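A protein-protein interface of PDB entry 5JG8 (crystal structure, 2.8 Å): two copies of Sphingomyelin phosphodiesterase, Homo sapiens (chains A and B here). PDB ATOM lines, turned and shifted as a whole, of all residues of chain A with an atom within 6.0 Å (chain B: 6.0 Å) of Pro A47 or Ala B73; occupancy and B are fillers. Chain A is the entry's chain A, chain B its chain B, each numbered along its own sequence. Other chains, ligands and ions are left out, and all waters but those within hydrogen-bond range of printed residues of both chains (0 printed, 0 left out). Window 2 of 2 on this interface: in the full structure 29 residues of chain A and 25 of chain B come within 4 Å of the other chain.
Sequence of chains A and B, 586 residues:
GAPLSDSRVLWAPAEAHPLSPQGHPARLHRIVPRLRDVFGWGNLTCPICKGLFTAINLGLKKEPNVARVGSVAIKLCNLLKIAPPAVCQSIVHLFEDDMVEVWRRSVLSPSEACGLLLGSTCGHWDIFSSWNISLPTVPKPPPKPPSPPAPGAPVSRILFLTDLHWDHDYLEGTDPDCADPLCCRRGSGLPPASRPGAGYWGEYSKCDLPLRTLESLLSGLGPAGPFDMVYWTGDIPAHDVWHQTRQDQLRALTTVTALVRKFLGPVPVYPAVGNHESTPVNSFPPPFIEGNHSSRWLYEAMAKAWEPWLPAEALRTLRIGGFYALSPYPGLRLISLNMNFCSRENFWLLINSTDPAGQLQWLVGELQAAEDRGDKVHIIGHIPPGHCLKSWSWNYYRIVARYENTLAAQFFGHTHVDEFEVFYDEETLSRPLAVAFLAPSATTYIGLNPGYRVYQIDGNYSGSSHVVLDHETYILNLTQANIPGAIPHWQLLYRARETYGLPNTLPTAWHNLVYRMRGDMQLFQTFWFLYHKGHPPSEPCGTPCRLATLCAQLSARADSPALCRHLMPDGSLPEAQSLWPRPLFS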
ATOM      1  N   ASN A  43      17.233  26.283 -21.921  1.00  0.00           N
ATOM      2  CA  ASN A  43      16.488  25.128 -21.436  1.00  0.00           C
ATOM      3  C   ASN A  43      15.920  25.332 -20.037  1.00  0.00           C
ATOM      4  O   ASN A  43      15.004  24.602 -19.643  1.00  0.00           O
ATOM      5  CB  ASN A  43      17.391  23.898 -21.442  1.00  0.00           C
ATOM      6  CG  ASN A  43      17.849  23.526 -22.830  1.00  0.00           C
ATOM      7  OD1 ASN A  43      19.019  23.683 -23.179  1.00  0.00           O
ATOM      8  ND2 ASN A  43      16.920  23.029 -23.632  1.00  0.00           N
ATOM      9  N   LEU A  44      16.454  26.285 -19.270  1.00  0.00           N
ATOM     10  CA  LEU A  44      16.019  26.463 -17.892  1.00  0.00           C
ATOM     11  C   LEU A  44      14.725  27.255 -17.762  1.00  0.00           C
ATOM     12  O   LEU A  44      14.023  27.104 -16.756  1.00  0.00           O
ATOM     13  CB  LEU A  44      17.110  27.173 -17.088  1.00  0.00           C
ATOM     14  CG  LEU A  44      18.309  26.339 -16.649  1.00  0.00           C
ATOM     15  CD1 LEU A  44      19.118  27.113 -15.622  1.00  0.00           C
ATOM     16  CD2 LEU A  44      17.864  24.994 -16.098  1.00  0.00           C
ATOM     17  N   THR A  45      14.392  28.085 -18.754  1.00  0.00           N
ATOM     18  CA  THR A  45      13.232  28.964 -18.635  1.00  0.00           C
ATOM     19  C   THR A  45      11.977  28.188 -18.249  1.00  0.00           C
ATOM     20  O   THR A  45      11.265  28.562 -17.310  1.00  0.00           O
ATOM     21  CB  THR A  45      13.018  29.717 -19.947  1.00  0.00           C
ATOM     22  OG1 THR A  45      12.925  28.778 -21.026  1.00  0.00           O
ATOM     23  CG2 THR A  45      14.179  30.667 -20.206  1.00  0.00           C
ATOM     24  N   CYS A  46      11.697  27.093 -18.962  1.00  0.00           N
ATOM     25  CA  CYS A  46      10.503  26.300 -18.672  1.00  0.00           C
ATOM     26  C   CYS A  46      10.515  25.734 -17.259  1.00  0.00           C
ATOM     27  O   CYS A  46       9.567  25.993 -16.496  1.00  0.00           O
ATOM     28  CB  CYS A  46      10.356  25.203 -19.728  1.00  0.00           C
ATOM     29  SG  CYS A  46       8.942  24.095 -19.484  1.00  0.00           S
ATOM     30  N   PRO A  47      11.524  24.959 -16.847  1.00  0.00           N
ATOM     31  CA  PRO A  47      11.519  24.440 -15.470  1.00  0.00           C
ATOM     32  C   PRO A  47      11.428  25.526 -14.416  1.00  0.00           C
ATOM     33  O   PRO A  47      10.696  25.365 -13.432  1.00  0.00           O
ATOM     34  CB  PRO A  47      12.845  23.672 -15.390  1.00  0.00           C
ATOM     35  CG  PRO A  47      13.117  23.267 -16.800  1.00  0.00           C
ATOM     36  CD  PRO A  47      12.638  24.415 -17.640  1.00  0.00           C
ATOM     37  N   ILE A  48      12.150  26.636 -14.589  1.00  0.00           N
ATOM     38  CA  ILE A  48      12.045  27.729 -13.629  1.00  0.00           C
ATOM     39  C   ILE A  48      10.623  28.269 -13.590  1.00  0.00           C
ATOM     40  O   ILE A  48      10.124  28.665 -12.530  1.00  0.00           O
ATOM     41  CB  ILE A  48      13.062  28.837 -13.951  1.00  0.00           C
ATOM     42  CG1 ILE A  48      14.471  28.371 -13.588  1.00  0.00           C
ATOM     43  CG2 ILE A  48      12.721  30.105 -13.189  1.00  0.00           C
ATOM     44  CD1 ILE A  48      14.603  27.908 -12.154  1.00  0.00           C
ATOM     45  N   CYS A  49       9.947  28.301 -14.741  1.00  0.00           N
ATOM     46  CA  CYS A  49       8.559  28.752 -14.759  1.00  0.00           C
ATOM     47  C   CYS A  49       7.668  27.799 -13.970  1.00  0.00           C
ATOM     48  O   CYS A  49       6.948  28.217 -13.053  1.00  0.00           O
ATOM     49  CB  CYS A  49       8.069  28.893 -16.204  1.00  0.00           C
ATOM     50  SG  CYS A  49       6.394  29.572 -16.351  1.00  0.00           S
ATOM     51  N   LYS A  50       7.716  26.506 -14.304  1.00  0.00           N
ATOM     52  CA  LYS A  50       6.857  25.536 -13.630  1.00  0.00           C
ATOM     53  C   LYS A  50       7.093  25.541 -12.124  1.00  0.00           C
ATOM     54  O   LYS A  50       6.141  25.565 -11.336  1.00  0.00           O
ATOM     55  CB  LYS A  50       7.084  24.137 -14.205  1.00  0.00           C
ATOM     56  CG  LYS A  50       6.518  23.940 -15.595  1.00  0.00           C
ATOM     57  CD  LYS A  50       6.326  22.463 -15.903  1.00  0.00           C
ATOM     58  CE  LYS A  50       5.582  22.268 -17.216  1.00  0.00           C
ATOM     59  NZ  LYS A  50       5.298  20.832 -17.487  1.00  0.00           N
ATOM     60  N   GLY A  51       8.357  25.516 -11.703  1.00  0.00           N
ATOM     61  CA  GLY A  51       8.642  25.620 -10.281  1.00  0.00           C
ATOM     62  C   GLY A  51       8.119  26.912  -9.683  1.00  0.00           C
ATOM     63  O   GLY A  51       7.576  26.924  -8.575  1.00  0.00           O
ATOM     64  N   LEU A  52       8.273  28.017 -10.414  1.00  0.00           N
ATOM     65  CA  LEU A  52       7.789  29.309  -9.940  1.00  0.00           C
ATOM     66  C   LEU A  52       6.298  29.255  -9.623  1.00  0.00           C
ATOM     67  O   LEU A  52       5.858  29.695  -8.551  1.00  0.00           O
ATOM     68  CB  LEU A  52       8.095  30.381 -10.987  1.00  0.00           C
ATOM     69  CG  LEU A  52       8.409  31.784 -10.470  1.00  0.00           C
ATOM     70  CD1 LEU A  52       9.431  31.720  -9.357  1.00  0.00           C
ATOM     71  CD2 LEU A  52       8.928  32.645 -11.609  1.00  0.00           C
ATOM     72  N   CYS A 122       6.361  24.207 -23.636  1.00  0.00           N
ATOM     73  CA  CYS A 122       6.180  24.282 -22.188  1.00  0.00           C
ATOM     74  C   CYS A 122       4.724  24.620 -21.889  1.00  0.00           C
ATOM     75  O   CYS A 122       4.268  25.728 -22.190  1.00  0.00           O
ATOM     76  CB  CYS A 122       7.127  25.319 -21.586  1.00  0.00           C
ATOM     77  SG  CYS A 122       7.311  25.272 -19.787  1.00  0.00           S
ATOM     78  N   ARG B  68      12.314  26.396  -3.019  1.00  0.00           N
ATOM     79  CA  ARG B  68      11.328  25.463  -3.561  1.00  0.00           C
ATOM     80  C   ARG B  68      11.290  25.509  -5.086  1.00  0.00           C
ATOM     81  O   ARG B  68      11.346  24.466  -5.753  1.00  0.00           O
ATOM     82  CB  ARG B  68       9.949  25.761  -2.970  1.00  0.00           C
ATOM     83  CG  ARG B  68       9.825  25.379  -1.507  1.00  0.00           C
ATOM     84  CD  ARG B  68       8.418  25.601  -0.983  1.00  0.00           C
ATOM     85  NE  ARG B  68       8.318  25.271   0.437  1.00  0.00           N
ATOM     86  CZ  ARG B  68       8.654  26.097   1.422  1.00  0.00           C
ATOM     87  NH1 ARG B  68       9.113  27.310   1.147  1.00  0.00           N
ATOM     88  NH2 ARG B  68       8.531  25.710   2.686  1.00  0.00           N
ATOM     89  N   VAL B  69      11.180  26.712  -5.660  1.00  0.00           N
ATOM     90  CA  VAL B  69      11.200  26.830  -7.115  1.00  0.00           C
ATOM     91  C   VAL B  69      12.481  26.226  -7.671  1.00  0.00           C
ATOM     92  O   VAL B  69      12.461  25.514  -8.684  1.00  0.00           O
ATOM     93  CB  VAL B  69      11.024  28.299  -7.549  1.00  0.00           C
ATOM     94  CG1 VAL B  69       9.862  28.939  -6.810  1.00  0.00           C
ATOM     95  CG2 VAL B  69      12.302  29.090  -7.321  1.00  0.00           C
ATOM     96  N   GLY B  70      13.611  26.480  -7.008  1.00  0.00           N
ATOM     97  CA  GLY B  70      14.866  25.896  -7.452  1.00  0.00           C
ATOM     98  C   GLY B  70      14.814  24.381  -7.514  1.00  0.00           C
ATOM     99  O   GLY B  70      15.250  23.774  -8.493  1.00  0.00           O
ATOM    100  N   SER B  71      14.289  23.749  -6.459  1.00  0.00           N
ATOM    101  CA  SER B  71      14.276  22.290  -6.395  1.00  0.00           C
ATOM    102  C   SER B  71      13.320  21.696  -7.424  1.00  0.00           C
ATOM    103  O   SER B  71      13.640  20.686  -8.069  1.00  0.00           O
ATOM    104  CB  SER B  71      13.910  21.831  -4.984  1.00  0.00           C
ATOM    105  OG  SER B  71      12.643  22.333  -4.597  1.00  0.00           O
ATOM    106  N   VAL B  72      12.138  22.300  -7.589  1.00  0.00           N
ATOM    107  CA  VAL B  72      11.230  21.844  -8.638  1.00  0.00           C
ATOM    108  C   VAL B  72      11.907  21.955  -9.997  1.00  0.00           C
ATOM    109  O   VAL B  72      11.826  21.044 -10.832  1.00  0.00           O
ATOM    110  CB  VAL B  72       9.913  22.642  -8.597  1.00  0.00           C
ATOM    111  CG1 VAL B  72       8.942  22.112  -9.644  1.00  0.00           C
ATOM    112  CG2 VAL B  72       9.299  22.592  -7.207  1.00  0.00           C
ATOM    113  N   ALA B  73      12.592  23.077 -10.235  1.00  0.00           N
ATOM    114  CA  ALA B  73      13.328  23.251 -11.481  1.00  0.00           C
ATOM    115  C   ALA B  73      14.405  22.187 -11.643  1.00  0.00           C
ATOM    116  O   ALA B  73      14.665  21.726 -12.759  1.00  0.00           O
ATOM    117  CB  ALA B  73      13.940  24.652 -11.538  1.00  0.00           C
ATOM    118  N   ILE B  74      15.052  21.789 -10.547  1.00  0.00           N
ATOM    119  CA  ILE B  74      16.075  20.750 -10.628  1.00  0.00           C
ATOM    120  C   ILE B  74      15.453  19.435 -11.074  1.00  0.00           C
ATOM    121  O   ILE B  74      15.950  18.767 -11.990  1.00  0.00           O
ATOM    122  CB  ILE B  74      16.799  20.598  -9.278  1.00  0.00           C
ATOM    123  CG1 ILE B  74      17.527  21.892  -8.920  1.00  0.00           C
ATOM    124  CG2 ILE B  74      17.757  19.414  -9.313  1.00  0.00           C
ATOM    125  CD1 ILE B  74      18.561  21.735  -7.823  1.00  0.00           C
ATOM    126  N   LYS B  75      14.347  19.051 -10.438  1.00  0.00           N
ATOM    127  CA  LYS B  75      13.682  17.814 -10.828  1.00  0.00           C
ATOM    128  C   LYS B  75      13.255  17.868 -12.291  1.00  0.00           C
ATOM    129  O   LYS B  75      13.377  16.874 -13.021  1.00  0.00           O
ATOM    130  CB  LYS B  75      12.486  17.555  -9.910  1.00  0.00           C
ATOM    131  CG  LYS B  75      12.872  17.427  -8.441  1.00  0.00           C
ATOM    132  CD  LYS B  75      11.714  16.952  -7.575  1.00  0.00           C
ATOM    133  CE  LYS B  75      12.167  16.727  -6.137  1.00  0.00           C
ATOM    134  NZ  LYS B  75      11.082  16.176  -5.277  1.00  0.00           N
ATOM    135  N   LEU B  76      12.774  19.029 -12.744  1.00  0.00           N
ATOM    136  CA  LEU B  76      12.365  19.170 -14.139  1.00  0.00           C
ATOM    137  C   LEU B  76      13.554  19.033 -15.086  1.00  0.00           C
ATOM    138  O   LEU B  76      13.474  18.330 -16.099  1.00  0.00           O
ATOM    139  CB  LEU B  76      11.666  20.516 -14.338  1.00  0.00           C
ATOM    140  CG  LEU B  76      10.349  20.699 -13.581  1.00  0.00           C
ATOM    141  CD1 LEU B  76       9.846  22.128 -13.725  1.00  0.00           C
ATOM    142  CD2 LEU B  76       9.299  19.701 -14.056  1.00  0.00           C
ATOM    143  N   CYS B  77      14.667  19.704 -14.772  1.00  0.00           N
ATOM    144  CA  CYS B  77      15.890  19.553 -15.557  1.00  0.00           C
ATOM    145  C   CYS B  77      16.267  18.085 -15.683  1.00  0.00           C
ATOM    146  O   CYS B  77      16.538  17.590 -16.783  1.00  0.00           O
ATOM    147  CB  CYS B  77      17.027  20.345 -14.907  1.00  0.00           C
ATOM    148  SG  CYS B  77      18.583  20.474 -15.857  1.00  0.00           S
ATOM    149  N   ASN B  78      16.280  17.369 -14.555  1.00  0.00           N
ATOM    150  CA  ASN B  78      16.543  15.936 -14.608  1.00  0.00           C
ATOM    151  C   ASN B  78      15.539  15.221 -15.501  1.00  0.00           C
ATOM    152  O   ASN B  78      15.884  14.223 -16.146  1.00  0.00           O
ATOM    153  CB  ASN B  78      16.525  15.346 -13.197  1.00  0.00           C
ATOM    154  CG  ASN B  78      17.616  15.920 -12.311  1.00  0.00           C
ATOM    155  OD1 ASN B  78      18.681  16.316 -12.791  1.00  0.00           O
ATOM    156  ND2 ASN B  78      17.356  15.969 -11.011  1.00  0.00           N
ATOM    157  N   LEU B  80      13.958  16.495 -18.300  1.00  0.00           N
ATOM    158  CA  LEU B  80      14.346  16.769 -19.681  1.00  0.00           C
ATOM    159  C   LEU B  80      15.714  16.195 -20.027  1.00  0.00           C
ATOM    160  O   LEU B  80      16.129  16.271 -21.190  1.00  0.00           O
ATOM    161  CB  LEU B  80      14.343  18.278 -19.945  1.00  0.00           C
ATOM    162  CG  LEU B  80      13.041  19.053 -19.725  1.00  0.00           C
ATOM    163  CD1 LEU B  80      13.218  20.515 -20.119  1.00  0.00           C
ATOM    164  CD2 LEU B  80      11.886  18.423 -20.489  1.00  0.00           C
ATOM    165  N   VAL B  92      21.134  25.504 -11.731  1.00  0.00           N
ATOM    166  CA  VAL B  92      19.915  26.086 -11.177  1.00  0.00           C
ATOM    167  C   VAL B  92      20.210  26.774  -9.851  1.00  0.00           C
ATOM    168  O   VAL B  92      19.694  27.861  -9.573  1.00  0.00           O
ATOM    169  CB  VAL B  92      18.824  25.013 -11.030  1.00  0.00           C
ATOM    170  CG1 VAL B  92      19.365  23.839 -10.255  1.00  0.00           C
ATOM    171  CG2 VAL B  92      17.604  25.596 -10.330  1.00  0.00           C
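The side-chain sulfur of Cys A46 is disulfide-bonded to the side-chain sulfur of Cys A122, at 2.0 Å.
Among the printed residues, merely in contact across the chains: Pro A47 with Leu B76, Ile A48 with Ala B73, Lys A50 with Leu B76, Gly A51 with Val B69, Gly A51 with Val B72, Pro A47 with Ala B73 and Leu A52 with Val B69.
Ala B73 touches just these residues of chain A: Pro A47 and Ile A48.
Printed residues of chain A within 4 Å of Val B72: Gly A51 (3.6 Å).
Printed residues of chain B within 4 Å of Ile A48: Ala B73 (3.4 Å).
Of the printed residues of chain A, Leu B76 touches Pro A47 and Lys A50.
Printed residues of chain B within 4 Å of Lys A50: Leu B76 (3.4 Å).
Ser B71 touches none of the printed residues of chain A.
Asn B78 touches none of the printed residues of chain A.
The nearest residue of chain A that does not touch Ala B73 is Gly A51 (4.7 Å).
Of the 11 printed residues of chain A, 5 touch a printed residue of chain B.
Printed residues of chain A that touch a printed residue of chain B: Pro A47, Ile A48, Lys A50, Gly A51 and Leu A52.
No position is printed for both chains.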
